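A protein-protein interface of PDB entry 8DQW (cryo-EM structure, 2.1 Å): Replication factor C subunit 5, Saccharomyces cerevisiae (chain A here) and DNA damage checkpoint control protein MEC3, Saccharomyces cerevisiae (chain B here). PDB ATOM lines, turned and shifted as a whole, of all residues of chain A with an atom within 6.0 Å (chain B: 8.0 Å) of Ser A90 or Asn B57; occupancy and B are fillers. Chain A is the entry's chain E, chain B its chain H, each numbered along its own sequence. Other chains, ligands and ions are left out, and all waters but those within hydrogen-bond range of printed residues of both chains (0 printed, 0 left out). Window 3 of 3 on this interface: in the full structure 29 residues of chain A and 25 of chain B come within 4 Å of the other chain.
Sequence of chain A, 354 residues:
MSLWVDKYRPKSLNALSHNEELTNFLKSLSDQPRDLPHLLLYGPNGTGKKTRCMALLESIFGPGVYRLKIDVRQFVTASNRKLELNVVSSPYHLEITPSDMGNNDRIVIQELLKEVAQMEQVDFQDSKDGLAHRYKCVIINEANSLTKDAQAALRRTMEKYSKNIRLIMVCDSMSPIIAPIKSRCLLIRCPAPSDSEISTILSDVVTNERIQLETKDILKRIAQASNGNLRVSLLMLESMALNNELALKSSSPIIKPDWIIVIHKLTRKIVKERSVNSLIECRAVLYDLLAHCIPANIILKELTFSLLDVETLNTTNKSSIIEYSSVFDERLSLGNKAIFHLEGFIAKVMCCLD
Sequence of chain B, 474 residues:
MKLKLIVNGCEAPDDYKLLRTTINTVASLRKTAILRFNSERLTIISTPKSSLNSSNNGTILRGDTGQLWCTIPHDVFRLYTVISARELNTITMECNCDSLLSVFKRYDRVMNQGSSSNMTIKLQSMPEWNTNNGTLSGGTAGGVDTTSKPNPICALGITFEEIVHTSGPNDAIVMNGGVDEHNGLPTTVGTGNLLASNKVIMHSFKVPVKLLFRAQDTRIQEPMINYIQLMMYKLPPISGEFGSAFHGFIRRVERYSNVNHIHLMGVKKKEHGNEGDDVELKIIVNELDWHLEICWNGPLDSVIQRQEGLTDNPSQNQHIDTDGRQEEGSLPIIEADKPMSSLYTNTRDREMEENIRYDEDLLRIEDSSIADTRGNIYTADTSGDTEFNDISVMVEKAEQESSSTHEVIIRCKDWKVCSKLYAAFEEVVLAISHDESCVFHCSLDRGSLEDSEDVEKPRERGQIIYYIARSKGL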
ATOM      1  N   GLY A  64     -27.185  21.947  19.858  1.00  0.00           N
ATOM      2  CA  GLY A  64     -26.073  21.210  20.429  1.00  0.00           C
ATOM      3  C   GLY A  64     -24.920  21.002  19.471  1.00  0.00           C
ATOM      4  O   GLY A  64     -23.812  20.678  19.909  1.00  0.00           O
ATOM      5  N   VAL A  65     -25.151  21.183  18.168  1.00  0.00           N
ATOM      6  CA  VAL A  65     -24.077  21.040  17.195  1.00  0.00           C
ATOM      7  C   VAL A  65     -22.980  22.067  17.428  1.00  0.00           C
ATOM      8  O   VAL A  65     -21.855  21.887  16.951  1.00  0.00           O
ATOM      9  CB  VAL A  65     -24.630  21.144  15.757  1.00  0.00           C
ATOM     10  CG1 VAL A  65     -25.733  20.116  15.529  1.00  0.00           C
ATOM     11  CG2 VAL A  65     -25.137  22.553  15.473  1.00  0.00           C
ATOM     12  N   TYR A  66     -23.273  23.145  18.153  1.00  0.00           N
ATOM     13  CA  TYR A  66     -22.285  24.177  18.433  1.00  0.00           C
ATOM     14  C   TYR A  66     -21.487  23.908  19.703  1.00  0.00           C
ATOM     15  O   TYR A  66     -20.593  24.695  20.031  1.00  0.00           O
ATOM     16  CB  TYR A  66     -22.971  25.543  18.526  1.00  0.00           C
ATOM     17  CG  TYR A  66     -23.548  26.009  17.209  1.00  0.00           C
ATOM     18  CD1 TYR A  66     -22.723  26.465  16.188  1.00  0.00           C
ATOM     19  CD2 TYR A  66     -24.918  25.979  16.979  1.00  0.00           C
ATOM     20  CE1 TYR A  66     -23.246  26.887  14.982  1.00  0.00           C
ATOM     21  CE2 TYR A  66     -25.449  26.399  15.775  1.00  0.00           C
ATOM     22  CZ  TYR A  66     -24.609  26.852  14.780  1.00  0.00           C
ATOM     23  OH  TYR A  66     -25.133  27.270  13.580  1.00  0.00           O
ATOM     24  N   ARG A  67     -21.780  22.821  20.417  1.00  0.00           N
ATOM     25  CA  ARG A  67     -21.026  22.433  21.610  1.00  0.00           C
ATOM     26  C   ARG A  67     -19.861  21.565  21.154  1.00  0.00           C
ATOM     27  O   ARG A  67     -19.929  20.335  21.171  1.00  0.00           O
ATOM     28  CB  ARG A  67     -21.922  21.699  22.598  1.00  0.00           C
ATOM     29  CG  ARG A  67     -22.936  22.587  23.303  1.00  0.00           C
ATOM     30  CD  ARG A  67     -23.399  21.966  24.612  1.00  0.00           C
ATOM     31  NE  ARG A  67     -24.197  20.765  24.391  1.00  0.00           N
ATOM     32  CZ  ARG A  67     -25.463  20.766  23.997  1.00  0.00           C
ATOM     33  NH1 ARG A  67     -26.120  21.894  23.777  1.00  0.00           N
ATOM     34  NH2 ARG A  67     -26.087  19.605  23.817  1.00  0.00           N
ATOM     35  N   LEU A  68     -18.773  22.213  20.755  1.00  0.00           N
ATOM     36  CA  LEU A  68     -17.648  21.542  20.122  1.00  0.00           C
ATOM     37  C   LEU A  68     -16.532  21.298  21.128  1.00  0.00           C
ATOM     38  O   LEU A  68     -16.299  22.115  22.024  1.00  0.00           O
ATOM     39  CB  LEU A  68     -17.110  22.372  18.954  1.00  0.00           C
ATOM     40  CG  LEU A  68     -18.139  22.807  17.908  1.00  0.00           C
ATOM     41  CD1 LEU A  68     -17.516  23.778  16.921  1.00  0.00           C
ATOM     42  CD2 LEU A  68     -18.713  21.600  17.187  1.00  0.00           C
ATOM     43  N   LYS A  69     -15.849  20.165  20.976  1.00  0.00           N
ATOM     44  CA  LYS A  69     -14.627  19.892  21.720  1.00  0.00           C
ATOM     45  C   LYS A  69     -13.608  19.300  20.759  1.00  0.00           C
ATOM     46  O   LYS A  69     -13.923  18.968  19.613  1.00  0.00           O
ATOM     47  CB  LYS A  69     -14.874  18.955  22.909  1.00  0.00           C
ATOM     48  CG  LYS A  69     -15.755  17.759  22.609  1.00  0.00           C
ATOM     49  CD  LYS A  69     -15.565  16.681  23.664  1.00  0.00           C
ATOM     50  CE  LYS A  69     -14.301  15.872  23.421  1.00  0.00           C
ATOM     51  NZ  LYS A  69     -13.696  15.393  24.695  1.00  0.00           N
ATOM     52  N   VAL A  88     -12.332  17.717  15.616  1.00  0.00           N
ATOM     53  CA  VAL A  88     -13.342  18.464  16.353  1.00  0.00           C
ATOM     54  C   VAL A  88     -14.621  17.644  16.355  1.00  0.00           C
ATOM     55  O   VAL A  88     -14.944  16.982  15.366  1.00  0.00           O
ATOM     56  CB  VAL A  88     -13.557  19.859  15.735  1.00  0.00           C
ATOM     57  CG1 VAL A  88     -14.928  20.411  16.104  1.00  0.00           C
ATOM     58  CG2 VAL A  88     -12.459  20.807  16.182  1.00  0.00           C
ATOM     59  N   SER A  89     -15.347  17.665  17.467  1.00  0.00           N
ATOM     60  CA  SER A  89     -16.519  16.818  17.605  1.00  0.00           C
ATOM     61  C   SER A  89     -17.624  17.546  18.352  1.00  0.00           C
ATOM     62  O   SER A  89     -17.364  18.305  19.291  1.00  0.00           O
ATOM     63  CB  SER A  89     -16.174  15.511  18.333  1.00  0.00           C
ATOM     64  OG  SER A  89     -15.473  15.767  19.537  1.00  0.00           O
ATOM     65  N   SER A  90     -18.850  17.307  17.911  1.00  0.00           N
ATOM     66  CA  SER A  90     -20.077  17.645  18.609  1.00  0.00           C
ATOM     67  C   SER A  90     -20.908  16.377  18.688  1.00  0.00           C
ATOM     68  O   SER A  90     -20.754  15.474  17.856  1.00  0.00           O
ATOM     69  CB  SER A  90     -20.864  18.744  17.882  1.00  0.00           C
ATOM     70  OG  SER A  90     -21.925  18.186  17.126  1.00  0.00           O
ATOM     71  N   PRO A  91     -21.822  16.285  19.653  1.00  0.00           N
ATOM     72  CA  PRO A  91     -22.543  15.019  19.864  1.00  0.00           C
ATOM     73  C   PRO A  91     -23.227  14.476  18.615  1.00  0.00           C
ATOM     74  O   PRO A  91     -23.693  13.332  18.620  1.00  0.00           O
ATOM     75  CB  PRO A  91     -23.570  15.371  20.951  1.00  0.00           C
ATOM     76  CG  PRO A  91     -23.620  16.862  21.000  1.00  0.00           C
ATOM     77  CD  PRO A  91     -22.287  17.351  20.556  1.00  0.00           C
ATOM     78  N   TYR A  92     -23.294  15.269  17.542  1.00  0.00           N
ATOM     79  CA  TYR A  92     -23.951  14.845  16.317  1.00  0.00           C
ATOM     80  C   TYR A  92     -23.056  14.831  15.085  1.00  0.00           C
ATOM     81  O   TYR A  92     -23.477  14.289  14.057  1.00  0.00           O
ATOM     82  CB  TYR A  92     -25.162  15.744  16.025  1.00  0.00           C
ATOM     83  CG  TYR A  92     -26.006  16.048  17.241  1.00  0.00           C
ATOM     84  CD1 TYR A  92     -25.855  17.244  17.931  1.00  0.00           C
ATOM     85  CD2 TYR A  92     -26.950  15.140  17.700  1.00  0.00           C
ATOM     86  CE1 TYR A  92     -26.625  17.528  19.042  1.00  0.00           C
ATOM     87  CE2 TYR A  92     -27.724  15.416  18.811  1.00  0.00           C
ATOM     88  CZ  TYR A  92     -27.557  16.610  19.478  1.00  0.00           C
ATOM     89  OH  TYR A  92     -28.323  16.890  20.586  1.00  0.00           O
ATOM     90  N   HIS A  93     -21.851  15.394  15.140  1.00  0.00           N
ATOM     91  CA  HIS A  93     -21.046  15.491  13.928  1.00  0.00           C
ATOM     92  C   HIS A  93     -19.568  15.602  14.283  1.00  0.00           C
ATOM     93  O   HIS A  93     -19.192  15.836  15.434  1.00  0.00           O
ATOM     94  CB  HIS A  93     -21.485  16.679  13.062  1.00  0.00           C
ATOM     95  CG  HIS A  93     -20.825  17.971  13.426  1.00  0.00           C
ATOM     96  ND1 HIS A  93     -21.259  18.762  14.468  1.00  0.00           N
ATOM     97  CD2 HIS A  93     -19.760  18.610  12.887  1.00  0.00           C
ATOM     98  CE1 HIS A  93     -20.491  19.834  14.554  1.00  0.00           C
ATOM     99  NE2 HIS A  93     -19.574  19.766  13.606  1.00  0.00           N
ATOM    100  N   LEU A  94     -18.737  15.421  13.259  1.00  0.00           N
ATOM    101  CA  LEU A  94     -17.290  15.516  13.373  1.00  0.00           C
ATOM    102  C   LEU A  94     -16.768  16.493  12.328  1.00  0.00           C
ATOM    103  O   LEU A  94     -17.405  16.735  11.303  1.00  0.00           O
ATOM    104  CB  LEU A  94     -16.613  14.149  13.187  1.00  0.00           C
ATOM    105  CG  LEU A  94     -17.206  12.976  13.970  1.00  0.00           C
ATOM    106  CD1 LEU A  94     -16.761  11.656  13.363  1.00  0.00           C
ATOM    107  CD2 LEU A  94     -16.810  13.058  15.433  1.00  0.00           C
ATOM    108  N   PRO B  48     -24.876   7.336  28.909  1.00  0.00           N
ATOM    109  CA  PRO B  48     -24.255   8.417  28.131  1.00  0.00           C
ATOM    110  C   PRO B  48     -25.165   9.611  27.899  1.00  0.00           C
ATOM    111  O   PRO B  48     -24.692  10.636  27.389  1.00  0.00           O
ATOM    112  CB  PRO B  48     -23.906   7.730  26.805  1.00  0.00           C
ATOM    113  CG  PRO B  48     -24.922   6.658  26.666  1.00  0.00           C
ATOM    114  CD  PRO B  48     -25.243   6.187  28.060  1.00  0.00           C
ATOM    115  N   LEU B  52     -23.372  15.519  32.079  1.00  0.00           N
ATOM    116  CA  LEU B  52     -21.915  15.487  32.143  1.00  0.00           C
ATOM    117  C   LEU B  52     -21.337  14.468  31.169  1.00  0.00           C
ATOM    118  O   LEU B  52     -20.343  14.748  30.488  1.00  0.00           O
ATOM    119  CB  LEU B  52     -21.460  15.180  33.571  1.00  0.00           C
ATOM    120  CG  LEU B  52     -21.871  16.192  34.644  1.00  0.00           C
ATOM    121  CD1 LEU B  52     -21.404  15.730  36.016  1.00  0.00           C
ATOM    122  CD2 LEU B  52     -21.320  17.575  34.328  1.00  0.00           C
ATOM    123  N   ASN B  53     -21.940  13.281  31.090  1.00  0.00           N
ATOM    124  CA  ASN B  53     -21.420  12.250  30.197  1.00  0.00           C
ATOM    125  C   ASN B  53     -21.539  12.668  28.736  1.00  0.00           C
ATOM    126  O   ASN B  53     -20.600  12.482  27.953  1.00  0.00           O
ATOM    127  CB  ASN B  53     -22.154  10.932  30.443  1.00  0.00           C
ATOM    128  CG  ASN B  53     -22.097  10.497  31.893  1.00  0.00           C
ATOM    129  OD1 ASN B  53     -23.047  10.689  32.650  1.00  0.00           O
ATOM    130  ND2 ASN B  53     -20.973   9.913  32.291  1.00  0.00           N
ATOM    131  N   SER B  54     -22.675  13.256  28.353  1.00  0.00           N
ATOM    132  CA  SER B  54     -22.876  13.637  26.961  1.00  0.00           C
ATOM    133  C   SER B  54     -21.875  14.688  26.502  1.00  0.00           C
ATOM    134  O   SER B  54     -21.723  14.896  25.294  1.00  0.00           O
ATOM    135  CB  SER B  54     -24.301  14.153  26.750  1.00  0.00           C
ATOM    136  OG  SER B  54     -25.250  13.324  27.396  1.00  0.00           O
ATOM    137  N   SER B  55     -21.192  15.352  27.433  1.00  0.00           N
ATOM    138  CA  SER B  55     -20.151  16.306  27.072  1.00  0.00           C
ATOM    139  C   SER B  55     -18.926  15.638  26.462  1.00  0.00           C
ATOM    140  O   SER B  55     -18.067  16.344  25.923  1.00  0.00           O
ATOM    141  CB  SER B  55     -19.735  17.116  28.301  1.00  0.00           C
ATOM    142  OG  SER B  55     -18.690  16.468  29.007  1.00  0.00           O
ATOM    143  N   ASN B  56     -18.815  14.311  26.537  1.00  0.00           N
ATOM    144  CA  ASN B  56     -17.687  13.596  25.958  1.00  0.00           C
ATOM    145  C   ASN B  56     -17.948  13.111  24.537  1.00  0.00           C
ATOM    146  O   ASN B  56     -17.004  12.674  23.870  1.00  0.00           O
ATOM    147  CB  ASN B  56     -17.315  12.396  26.838  1.00  0.00           C
ATOM    148  CG  ASN B  56     -16.379  12.771  27.970  1.00  0.00           C
ATOM    149  OD1 ASN B  56     -15.175  12.521  27.905  1.00  0.00           O
ATOM    150  ND2 ASN B  56     -16.928  13.378  29.016  1.00  0.00           N
ATOM    151  N   ASN B  57     -19.189  13.183  24.059  1.00  0.00           N
ATOM    152  CA  ASN B  57     -19.537  12.717  22.716  1.00  0.00           C
ATOM    153  C   ASN B  57     -19.094  11.270  22.512  1.00  0.00           C
ATOM    154  O   ASN B  57     -18.568  10.899  21.461  1.00  0.00           O
ATOM    155  CB  ASN B  57     -18.930  13.625  21.646  1.00  0.00           C
ATOM    156  CG  ASN B  57     -19.210  15.095  21.898  1.00  0.00           C
ATOM    157  OD1 ASN B  57     -18.361  15.950  21.648  1.00  0.00           O
ATOM    158  ND2 ASN B  57     -20.405  15.396  22.395  1.00  0.00           N
ATOM    159  N   GLY B  58     -19.311  10.443  23.535  1.00  0.00           N
ATOM    160  CA  GLY B  58     -18.875   9.058  23.457  1.00  0.00           C
ATOM    161  C   GLY B  58     -19.627   8.259  22.410  1.00  0.00           C
ATOM    162  O   GLY B  58     -19.038   7.435  21.706  1.00  0.00           O
ATOM    163  N   THR B  59     -20.934   8.495  22.285  1.00  0.00           N
ATOM    164  CA  THR B  59     -21.751   7.680  21.391  1.00  0.00           C
ATOM    165  C   THR B  59     -21.269   7.790  19.949  1.00  0.00           C
ATOM    166  O   THR B  59     -21.150   6.781  19.245  1.00  0.00           O
ATOM    167  CB  THR B  59     -23.218   8.099  21.499  1.00  0.00           C
ATOM    168  OG1 THR B  59     -23.653   7.981  22.859  1.00  0.00           O
ATOM    169  CG2 THR B  59     -24.094   7.226  20.610  1.00  0.00           C
ATOM    170  N   ILE B  60     -20.980   9.009  19.492  1.00  0.00           N
ATOM    171  CA  ILE B  60     -20.624   9.194  18.089  1.00  0.00           C
ATOM    172  C   ILE B  60     -19.165   8.832  17.828  1.00  0.00           C
ATOM    173  O   ILE B  60     -18.814   8.438  16.710  1.00  0.00           O
ATOM    174  CB  ILE B  60     -20.924  10.636  17.647  1.00  0.00           C
ATOM    175  CG1 ILE B  60     -20.784  10.761  16.128  1.00  0.00           C
ATOM    176  CG2 ILE B  60     -19.994  11.621  18.345  1.00  0.00           C
ATOM    177  CD1 ILE B  60     -21.433  11.997  15.553  1.00  0.00           C
ATOM    178  N   LEU B  61     -18.297   8.947  18.834  1.00  0.00           N
ATOM    179  CA  LEU B  61     -16.868   8.748  18.620  1.00  0.00           C
ATOM    180  C   LEU B  61     -16.430   7.305  18.833  1.00  0.00           C
ATOM    181  O   LEU B  61     -15.599   6.797  18.074  1.00  0.00           O
ATOM    182  CB  LEU B  61     -16.067   9.666  19.547  1.00  0.00           C
ATOM    183  CG  LEU B  61     -15.851  11.098  19.050  1.00  0.00           C
ATOM    184  CD1 LEU B  61     -15.449  12.002  20.203  1.00  0.00           C
ATOM    185  CD2 LEU B  61     -14.809  11.144  17.944  1.00  0.00           C
ATOM    186  N   ARG B  62     -16.961   6.629  19.857  1.00  0.00           N
ATOM    187  CA  ARG B  62     -16.526   5.281  20.198  1.00  0.00           C
ATOM    188  C   ARG B  62     -17.694   4.333  20.447  1.00  0.00           C
ATOM    189  O   ARG B  62     -17.469   3.201  20.889  1.00  0.00           O
ATOM    190  CB  ARG B  62     -15.611   5.300  21.432  1.00  0.00           C
ATOM    191  CG  ARG B  62     -14.714   6.528  21.558  1.00  0.00           C
ATOM    192  CD  ARG B  62     -14.205   6.696  22.982  1.00  0.00           C
ATOM    193  NE  ARG B  62     -13.555   7.988  23.182  1.00  0.00           N
ATOM    194  CZ  ARG B  62     -14.172   9.091  23.586  1.00  0.00           C
ATOM    195  NH1 ARG B  62     -15.470   9.104  23.845  1.00  0.00           N
ATOM    196  NH2 ARG B  62     -13.469  10.210  23.732  1.00  0.00           N
ATOM    197  N   GLY B  63     -18.926   4.759  20.182  1.00  0.00           N
ATOM    198  CA  GLY B  63     -20.077   3.895  20.354  1.00  0.00           C
ATOM    199  C   GLY B  63     -20.283   3.425  21.780  1.00  0.00           C
ATOM    200  O   GLY B  63     -20.508   2.234  22.017  1.00  0.00           O
ATOM    201  N   ASP B  64     -20.204   4.346  22.741  1.00  0.00           N
ATOM    202  CA  ASP B  64     -20.445   4.027  24.150  1.00  0.00           C
ATOM    203  C   ASP B  64     -21.941   4.143  24.404  1.00  0.00           C
ATOM    204  O   ASP B  64     -22.445   5.184  24.831  1.00  0.00           O
ATOM    205  CB  ASP B  64     -19.646   4.950  25.061  1.00  0.00           C
ATOM    206  CG  ASP B  64     -18.232   5.175  24.570  1.00  0.00           C
ATOM    207  OD1 ASP B  64     -18.067   5.825  23.517  1.00  0.00           O
ATOM    208  OD2 ASP B  64     -17.287   4.702  25.235  1.00  0.00           O
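Among the printed residues, pairs that only touch across the chains: Lys A69 with Ser B55 (3.4 Å), Lys A69 with Asn B57 (3.3 Å), Ser A89 with Leu B61 (3.8 Å), Ser A90 with Asn B57 (3.9 Å), Ser A90 with Ile B60 (3.96 Å), Pro A91 with Ile B60 (3.99 Å), Tyr A92 with Ile B60 (3.3 Å), His A93 with Ile B60 (3.4 Å) and Leu A94 with Leu B61 (3.7 Å).
ND2 of Asn B57 sits at hydrogen-bond distance from O of Ser B54 (3.2 Å). The side-chain hydroxyl of Ser A90 lies within hydrogen-bond range of a ring nitrogen (ND1) of His A93 (2.8 Å). The side-chain hydroxyl (OG) of Ser A90 sits close to the backbone NH (N) of Tyr A92 (3.2 Å). OG of Ser B55 is in hydrogen-bond range of O of Leu B52, 2.8 Å away. The backbone carbonyl oxygen (O) of Lys A69 is in hydrogen-bond range of the backbone NH (N) of Ser A89, 2.9 Å away.
Of the 14 printed residues of chain B, 4 touch a printed residue of chain A. Hydrophobic or aromatic side chains of chain B that line the printed part of chain A: Ile B60 and Leu B61. Of the 13 printed residues of chain A, 7 touch a printed residue of chain B. Among the printed residues, no Asp or Glu carboxylate lies within 4 Å of a Lys or Arg side-chain nitrogen of the other chain.
Of chain B, only Asn B57 and Ile B60 come within 4 Å of Ser A90. Ser A89 touches just these residues of chain B: Asn B57 and Leu B61. Of the printed residues of chain B, Tyr A92 touches Ile B60. Of the printed residues of chain B, His A93 touches Ile B60. Of the printed residues of chain B, Lys A69 touches Ser B55 (3.4 Å) and Asn B57 (3.3 Å). Of the printed residues of chain A, Ile B60 touches Ser A90 (3.96 Å), Pro A91 (3.99 Å), Tyr A92 (3.3 Å) and His A93 (3.4 Å). Of the printed residues of chain A, Ser B55 touches Lys A69. Ser B54 touches none of the printed residues of chain A. The nearest residue of chain B that does not touch Ser A90 is Leu B61 (6.7 Å). The nearest residue of chain A that does not touch Asn B57 is Arg A67 (4.7 Å). The nearest printed residue of chain B that does not touch Lys A69 is Asn B56 (4.2 Å).
O of Ser A89 lies close to OD1 of Asn B57 (3.5 Å). The backbone nitrogen (N) of Pro A91 lies close to the side-chain amide nitrogen (ND2) of Asn B57 (3.2 Å).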
